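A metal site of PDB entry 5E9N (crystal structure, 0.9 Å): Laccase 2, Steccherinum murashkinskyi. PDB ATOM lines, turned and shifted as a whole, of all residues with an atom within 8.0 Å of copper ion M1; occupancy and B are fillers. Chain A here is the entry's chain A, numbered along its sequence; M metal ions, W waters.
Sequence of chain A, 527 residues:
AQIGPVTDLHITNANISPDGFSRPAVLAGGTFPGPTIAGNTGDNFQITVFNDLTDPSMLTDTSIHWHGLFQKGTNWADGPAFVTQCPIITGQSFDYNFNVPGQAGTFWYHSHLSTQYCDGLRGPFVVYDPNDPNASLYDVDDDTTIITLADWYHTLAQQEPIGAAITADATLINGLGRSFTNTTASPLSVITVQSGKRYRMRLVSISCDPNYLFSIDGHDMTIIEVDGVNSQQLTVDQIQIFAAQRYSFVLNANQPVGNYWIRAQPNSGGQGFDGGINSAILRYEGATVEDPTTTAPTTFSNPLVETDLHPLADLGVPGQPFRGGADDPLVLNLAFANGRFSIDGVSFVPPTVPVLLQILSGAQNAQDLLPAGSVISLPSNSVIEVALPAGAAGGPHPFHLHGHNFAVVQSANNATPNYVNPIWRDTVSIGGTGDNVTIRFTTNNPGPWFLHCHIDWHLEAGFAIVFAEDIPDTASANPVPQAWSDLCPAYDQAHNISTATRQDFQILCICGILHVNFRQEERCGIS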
ATOM      1  N   HIS A  65      13.426   1.737  24.228  1.00  0.00           N
ATOM      2  CA  HIS A  65      13.838   1.131  25.464  1.00  0.00           C
ATOM      3  C   HIS A  65      15.332   0.929  25.447  1.00  0.00           C
ATOM      4  O   HIS A  65      15.948   0.559  24.454  1.00  0.00           O
ATOM      5  CB  HIS A  65      13.149  -0.195  25.613  1.00  0.00           C
ATOM      6  CG  HIS A  65      13.607  -1.037  26.763  1.00  0.00           C
ATOM      7  ND1 HIS A  65      13.582  -0.648  28.055  1.00  0.00           N
ATOM      8  CD2 HIS A  65      14.002  -2.312  26.793  1.00  0.00           C
ATOM      9  CE1 HIS A  65      13.996  -1.626  28.823  1.00  0.00           C
ATOM     10  NE2 HIS A  65      14.254  -2.670  28.080  1.00  0.00           N
ATOM     11  N   HIS A  67      17.776  -1.281  26.854  1.00  0.00           N
ATOM     12  CA  HIS A  67      17.653  -2.629  27.362  1.00  0.00           C
ATOM     13  C   HIS A  67      18.708  -2.939  28.373  1.00  0.00           C
ATOM     14  O   HIS A  67      19.881  -2.943  28.086  1.00  0.00           O
ATOM     15  CB  HIS A  67      17.732  -3.599  26.210  1.00  0.00           C
ATOM     16  CG  HIS A  67      17.595  -5.006  26.650  1.00  0.00           C
ATOM     17  ND1 HIS A  67      16.527  -5.796  26.315  1.00  0.00           N
ATOM     18  CD2 HIS A  67      18.411  -5.722  27.480  1.00  0.00           C
ATOM     19  CE1 HIS A  67      16.738  -6.974  26.899  1.00  0.00           C
ATOM     20  NE2 HIS A  67      17.850  -6.941  27.609  1.00  0.00           N
ATOM     21  N   ASP A  78      11.928   4.411  30.611  1.00  0.00           N
ATOM     22  CA  ASP A  78      12.268   3.044  30.272  1.00  0.00           C
ATOM     23  C   ASP A  78      11.914   2.675  28.863  1.00  0.00           C
ATOM     24  O   ASP A  78      12.553   1.804  28.279  1.00  0.00           O
ATOM     25  CB  ASP A  78      11.604   2.118  31.268  1.00  0.00           C
ATOM     26  CG  ASP A  78      12.063   0.677  31.193  1.00  0.00           C
ATOM     27  OD1 ASP A  78      13.280   0.454  31.069  1.00  0.00           O
ATOM     28  OD2 ASP A  78      11.196  -0.207  31.288  1.00  0.00           O
ATOM     29  N   GLY A  79      10.847   3.242  28.298  1.00  0.00           N
ATOM     30  CA  GLY A  79      10.483   3.030  26.927  1.00  0.00           C
ATOM     31  C   GLY A  79       9.373   2.068  26.544  1.00  0.00           C
ATOM     32  O   GLY A  79       8.914   2.226  25.442  1.00  0.00           O
ATOM     33  N   PRO A  80       8.994   1.059  27.304  1.00  0.00           N
ATOM     34  CA  PRO A  80       7.961   0.184  26.750  1.00  0.00           C
ATOM     35  C   PRO A  80       6.640   0.905  26.593  1.00  0.00           C
ATOM     36  O   PRO A  80       6.061   1.402  27.564  1.00  0.00           O
ATOM     37  CB  PRO A  80       7.898  -0.970  27.707  1.00  0.00           C
ATOM     38  CG  PRO A  80       8.424  -0.397  29.018  1.00  0.00           C
ATOM     39  CD  PRO A  80       9.517   0.569  28.571  1.00  0.00           C
ATOM     40  N   ALA A  81       6.145   0.924  25.378  1.00  0.00           N
ATOM     41  CA  ALA A  81       4.917   1.649  25.108  1.00  0.00           C
ATOM     42  C   ALA A  81       3.773   1.056  25.891  1.00  0.00           C
ATOM     43  O   ALA A  81       3.578  -0.140  25.944  1.00  0.00           O
ATOM     44  CB  ALA A  81       4.624   1.596  23.619  1.00  0.00           C
ATOM     45  N   VAL A  83       3.454   0.828  28.915  1.00  0.00           N
ATOM     46  CA  VAL A  83       3.859   0.437  30.229  1.00  0.00           C
ATOM     47  C   VAL A  83       4.399   1.646  30.953  1.00  0.00           C
ATOM     48  O   VAL A  83       3.919   1.986  32.030  1.00  0.00           O
ATOM     49  CB  VAL A  83       4.842  -0.754  30.222  1.00  0.00           C
ATOM     50  CG1 VAL A  83       5.243  -1.142  31.621  1.00  0.00           C
ATOM     51  CG2 VAL A  83       4.220  -1.915  29.480  1.00  0.00           C
ATOM     52  N   HIS A 110      16.317  -0.290  21.561  1.00  0.00           N
ATOM     53  CA  HIS A 110      15.418  -0.744  20.527  1.00  0.00           C
ATOM     54  C   HIS A 110      14.090  -0.109  20.686  1.00  0.00           C
ATOM     55  O   HIS A 110      13.651   0.239  21.781  1.00  0.00           O
ATOM     56  CB  HIS A 110      15.309  -2.246  20.494  1.00  0.00           C
ATOM     57  CG  HIS A 110      14.871  -2.911  21.755  1.00  0.00           C
ATOM     58  ND1 HIS A 110      13.565  -3.054  22.121  1.00  0.00           N
ATOM     59  CD2 HIS A 110      15.595  -3.538  22.716  1.00  0.00           C
ATOM     60  CE1 HIS A 110      13.519  -3.769  23.251  1.00  0.00           C
ATOM     61  NE2 HIS A 110      14.731  -4.087  23.627  1.00  0.00           N
ATOM     62  N   SER A 111      13.369   0.002  19.561  1.00  0.00           N
ATOM     63  CA  SER A 111      11.971   0.372  19.685  1.00  0.00           C
ATOM     64  C   SER A 111      11.262  -0.598  20.616  1.00  0.00           C
ATOM     65  O   SER A 111      11.544  -1.798  20.615  1.00  0.00           O
ATOM     66  CB  SER A 111      11.268   0.320  18.353  1.00  0.00           C
ATOM     67  OG  SER A 111       9.935   0.695  18.557  1.00  0.00           O
ATOM     68  N   HIS A 112      10.328  -0.064  21.376  1.00  0.00           N
ATOM     69  CA  HIS A 112       9.504  -0.868  22.251  1.00  0.00           C
ATOM     70  C   HIS A 112       8.052  -0.540  22.027  1.00  0.00           C
ATOM     71  O   HIS A 112       7.255  -0.485  22.973  1.00  0.00           O
ATOM     72  CB  HIS A 112       9.954  -0.751  23.705  1.00  0.00           C
ATOM     73  CG  HIS A 112       9.730  -1.969  24.506  1.00  0.00           C
ATOM     74  ND1 HIS A 112       8.585  -2.682  24.520  1.00  0.00           N
ATOM     75  CD2 HIS A 112      10.555  -2.657  25.320  1.00  0.00           C
ATOM     76  CE1 HIS A 112       8.749  -3.740  25.302  1.00  0.00           C
ATOM     77  NE2 HIS A 112       9.978  -3.763  25.814  1.00  0.00           N
ATOM     78  N   TYR A 117      10.880  -2.717  16.398  1.00  0.00           N
ATOM     79  CA  TYR A 117      12.312  -2.849  16.368  1.00  0.00           C
ATOM     80  C   TYR A 117      12.737  -3.806  15.284  1.00  0.00           C
ATOM     81  O   TYR A 117      13.842  -3.692  14.756  1.00  0.00           O
ATOM     82  CB  TYR A 117      12.950  -3.137  17.719  1.00  0.00           C
ATOM     83  CG  TYR A 117      13.100  -4.538  18.252  1.00  0.00           C
ATOM     84  CD1 TYR A 117      14.098  -5.392  17.791  1.00  0.00           C
ATOM     85  CD2 TYR A 117      12.408  -4.971  19.352  1.00  0.00           C
ATOM     86  CE1 TYR A 117      14.340  -6.606  18.368  1.00  0.00           C
ATOM     87  CE2 TYR A 117      12.661  -6.170  19.942  1.00  0.00           C
ATOM     88  CZ  TYR A 117      13.638  -6.997  19.467  1.00  0.00           C
ATOM     89  OH  TYR A 117      13.833  -8.173  20.109  1.00  0.00           O
ATOM     90  N   HIS A 400      12.720 -11.717  29.616  1.00  0.00           N
ATOM     91  CA  HIS A 400      13.447 -10.533  29.988  1.00  0.00           C
ATOM     92  C   HIS A 400      12.605  -9.742  30.966  1.00  0.00           C
ATOM     93  O   HIS A 400      11.429  -9.592  30.800  1.00  0.00           O
ATOM     94  CB  HIS A 400      13.724  -9.707  28.752  1.00  0.00           C
ATOM     95  CG  HIS A 400      14.243  -8.352  29.040  1.00  0.00           C
ATOM     96  ND1 HIS A 400      15.384  -8.120  29.768  1.00  0.00           N
ATOM     97  CD2 HIS A 400      13.787  -7.146  28.691  1.00  0.00           C
ATOM     98  CE1 HIS A 400      15.579  -6.826  29.860  1.00  0.00           C
ATOM     99  NE2 HIS A 400      14.617  -6.196  29.221  1.00  0.00           N
ATOM    100  N   LEU A 401      13.282  -9.213  31.991  1.00  0.00           N
ATOM    101  CA  LEU A 401      12.684  -8.375  33.021  1.00  0.00           C
ATOM    102  C   LEU A 401      13.347  -6.997  32.936  1.00  0.00           C
ATOM    103  O   LEU A 401      14.544  -6.888  32.998  1.00  0.00           O
ATOM    104  CB  LEU A 401      12.964  -8.957  34.372  1.00  0.00           C
ATOM    105  CG  LEU A 401      12.468  -8.153  35.566  1.00  0.00           C
ATOM    106  CD1 LEU A 401      10.990  -7.973  35.534  1.00  0.00           C
ATOM    107  CD2 LEU A 401      12.874  -8.849  36.856  1.00  0.00           C
ATOM    108  N   HIS A 402      12.497  -5.979  32.799  1.00  0.00           N
ATOM    109  CA  HIS A 402      12.960  -4.612  32.870  1.00  0.00           C
ATOM    110  C   HIS A 402      13.296  -4.235  34.300  1.00  0.00           C
ATOM    111  O   HIS A 402      12.817  -4.834  35.257  1.00  0.00           O
ATOM    112  CB  HIS A 402      11.893  -3.682  32.354  1.00  0.00           C
ATOM    113  CG  HIS A 402      11.603  -3.769  30.902  1.00  0.00           C
ATOM    114  ND1 HIS A 402      11.323  -2.639  30.196  1.00  0.00           N
ATOM    115  CD2 HIS A 402      11.491  -4.781  30.012  1.00  0.00           C
ATOM    116  CE1 HIS A 402      11.068  -2.959  28.935  1.00  0.00           C
ATOM    117  NE2 HIS A 402      11.131  -4.265  28.797  1.00  0.00           N
ATOM    118  N   TRP A 449       7.540  -2.648  35.784  1.00  0.00           N
ATOM    119  CA  TRP A 449       8.605  -3.280  35.005  1.00  0.00           C
ATOM    120  C   TRP A 449       8.036  -4.394  34.179  1.00  0.00           C
ATOM    121  O   TRP A 449       7.429  -5.337  34.690  1.00  0.00           O
ATOM    122  CB  TRP A 449       9.704  -3.778  35.906  1.00  0.00           C
ATOM    123  CG  TRP A 449      10.312  -2.678  36.729  1.00  0.00           C
ATOM    124  CD1 TRP A 449      10.265  -2.599  38.077  1.00  0.00           C
ATOM    125  CD2 TRP A 449      10.952  -1.477  36.277  1.00  0.00           C
ATOM    126  NE1 TRP A 449      10.833  -1.437  38.482  1.00  0.00           N
ATOM    127  CE2 TRP A 449      11.254  -0.730  37.411  1.00  0.00           C
ATOM    128  CE3 TRP A 449      11.333  -0.982  35.039  1.00  0.00           C
ATOM    129  CZ2 TRP A 449      11.910   0.486  37.354  1.00  0.00           C
ATOM    130  CZ3 TRP A 449      12.018   0.205  34.967  1.00  0.00           C
ATOM    131  CH2 TRP A 449      12.293   0.939  36.133  1.00  0.00           C
ATOM    132  N   PHE A 450       8.247  -4.314  32.885  1.00  0.00           N
ATOM    133  CA  PHE A 450       7.773  -5.337  31.985  1.00  0.00           C
ATOM    134  C   PHE A 450       8.540  -6.623  32.181  1.00  0.00           C
ATOM    135  O   PHE A 450       9.744  -6.609  32.346  1.00  0.00           O
ATOM    136  CB  PHE A 450       7.930  -4.817  30.557  1.00  0.00           C
ATOM    137  CG  PHE A 450       6.823  -5.050  29.593  1.00  0.00           C
ATOM    138  CD1 PHE A 450       5.626  -5.697  29.892  1.00  0.00           C
ATOM    139  CD2 PHE A 450       6.941  -4.510  28.336  1.00  0.00           C
ATOM    140  CE1 PHE A 450       4.629  -5.774  28.942  1.00  0.00           C
ATOM    141  CE2 PHE A 450       5.927  -4.606  27.424  1.00  0.00           C
ATOM    142  CZ  PHE A 450       4.780  -5.238  27.719  1.00  0.00           C
ATOM    143  N   LEU A 451       7.843  -7.745  32.096  1.00  0.00           N
ATOM    144  CA  LEU A 451       8.413  -9.078  32.044  1.00  0.00           C
ATOM    145  C   LEU A 451       7.814  -9.747  30.828  1.00  0.00           C
ATOM    146  O   LEU A 451       6.605  -9.893  30.732  1.00  0.00           O
ATOM    147  CB  LEU A 451       8.045  -9.906  33.272  1.00  0.00           C
ATOM    148  CG  LEU A 451       8.535 -11.332  33.209  1.00  0.00           C
ATOM    149  CD1 LEU A 451      10.010 -11.458  33.360  1.00  0.00           C
ATOM    150  CD2 LEU A 451       7.842 -12.207  34.241  1.00  0.00           C
ATOM    151  N   HIS A 452       8.655 -10.169  29.893  1.00  0.00           N
ATOM    152  CA  HIS A 452       8.104 -10.711  28.668  1.00  0.00           C
ATOM    153  C   HIS A 452       9.116 -11.560  27.964  1.00  0.00           C
ATOM    154  O   HIS A 452      10.308 -11.420  28.125  1.00  0.00           O
ATOM    155  CB  HIS A 452       7.610  -9.619  27.751  1.00  0.00           C
ATOM    156  CG  HIS A 452       8.652  -8.647  27.301  1.00  0.00           C
ATOM    157  ND1 HIS A 452       9.398  -8.844  26.172  1.00  0.00           N
ATOM    158  CD2 HIS A 452       9.057  -7.470  27.802  1.00  0.00           C
ATOM    159  CE1 HIS A 452      10.230  -7.814  26.025  1.00  0.00           C
ATOM    160  NE2 HIS A 452      10.038  -6.937  26.990  1.00  0.00           N
ATOM    161  N   CYS A 453       8.602 -12.406  27.096  1.00  0.00           N
ATOM    162  CA  CYS A 453       9.453 -13.049  26.119  1.00  0.00           C
ATOM    163  C   CYS A 453      10.019 -12.003  25.174  1.00  0.00           C
ATOM    164  O   CYS A 453       9.256 -11.174  24.691  1.00  0.00           O
ATOM    165  CB  CYS A 453       8.688 -14.085  25.354  1.00  0.00           C
ATOM    166  SG  CYS A 453       9.786 -14.910  24.176  1.00  0.00           S
ATOM    167  N   HIS A 454      11.304 -12.054  24.903  1.00  0.00           N
ATOM    168  CA  HIS A 454      11.916 -11.083  24.022  1.00  0.00           C
ATOM    169  C   HIS A 454      11.899 -11.485  22.570  1.00  0.00           C
ATOM    170  O   HIS A 454      12.397 -10.746  21.755  1.00  0.00           O
ATOM    171  CB  HIS A 454      13.329 -10.744  24.500  1.00  0.00           C
ATOM    172  CG  HIS A 454      13.691  -9.319  24.264  1.00  0.00           C
ATOM    173  ND1 HIS A 454      13.790  -8.742  23.028  1.00  0.00           N
ATOM    174  CD2 HIS A 454      14.043  -8.333  25.137  1.00  0.00           C
ATOM    175  CE1 HIS A 454      14.120  -7.465  23.190  1.00  0.00           C
ATOM    176  NE2 HIS A 454      14.306  -7.181  24.464  1.00  0.00           N
ATOM    177  N   ASP A 456      10.010 -10.888  19.691  1.00  0.00           N
ATOM    178  CA  ASP A 456       9.121  -9.742  19.594  1.00  0.00           C
ATOM    179  C   ASP A 456       7.766 -10.167  19.087  1.00  0.00           C
ATOM    180  O   ASP A 456       6.726  -9.598  19.477  1.00  0.00           O
ATOM    181  CB  ASP A 456       9.743  -8.664  18.729  1.00  0.00           C
ATOM    182  CG  ASP A 456       9.395  -7.268  19.245  1.00  0.00           C
ATOM    183  OD1 ASP A 456       9.246  -7.040  20.452  1.00  0.00           O
ATOM    184  OD2 ASP A 456       9.338  -6.360  18.398  1.00  0.00           O
ATOM    185  N   LEU A 459       5.909 -11.372  22.213  1.00  0.00           N
ATOM    186  CA  LEU A 459       5.440 -10.223  22.973  1.00  0.00           C
ATOM    187  C   LEU A 459       4.187  -9.661  22.335  1.00  0.00           C
ATOM    188  O   LEU A 459       3.188  -9.407  22.990  1.00  0.00           O
ATOM    189  CB  LEU A 459       6.538  -9.195  23.049  1.00  0.00           C
ATOM    190  CG  LEU A 459       6.133  -7.842  23.599  1.00  0.00           C
ATOM    191  CD1 LEU A 459       5.517  -7.931  24.971  1.00  0.00           C
ATOM    192  CD2 LEU A 459       7.315  -6.880  23.579  1.00  0.00           C
ATOM    193  N   ALA A 464       3.517 -11.582  28.039  1.00  0.00           N
ATOM    194  CA  ALA A 464       4.010 -10.537  28.915  1.00  0.00           C
ATOM    195  C   ALA A 464       3.116 -10.341  30.082  1.00  0.00           C
ATOM    196  O   ALA A 464       1.931 -10.570  30.017  1.00  0.00           O
ATOM    197  CB  ALA A 464       4.135  -9.242  28.153  1.00  0.00           C
HETATM  198 CU    CU M   1      10.505  -5.121  27.164  1.00  0.00          CU
HETATM  199 CU    CU M   2      14.540  -4.381  28.794  1.00  0.00          CU
HETATM  200 CU    CU M   3      15.305  -5.432  24.930  1.00  0.00          CU
HETATM  201  O   HOH W   1      12.625  -5.320  25.912  1.00  0.00           O
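Merely in contact with copper ion M1: Phe 450 (3.8 Å). Of the 23 residues printed, 4 come within 4 Å of copper ion M1.
Copper ion M1 is bound by NE2 of His 452 (1.9 Å), NE2 of His 402 (1.9 Å), NE2 of His 112 (2.0 Å) and water W1 (2.5 Å). Copper ion M1 has four donor atoms within binding distance.
A ring nitrogen (ND1) of His 402 sits at hydrogen-bond distance from the side-chain carboxylate (OD2) of Asp 78. The backbone NH (N) of Ala 81 lies within hydrogen-bond range of the backbone carbonyl oxygen (O) of His 112 (3.0 Å). O of Phe 450 sits at hydrogen-bond distance from N of His 402 (2.9 Å). The backbone NH of His 400 sits at hydrogen-bond distance from the backbone carbonyl oxygen of His 452 (2.9 Å).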
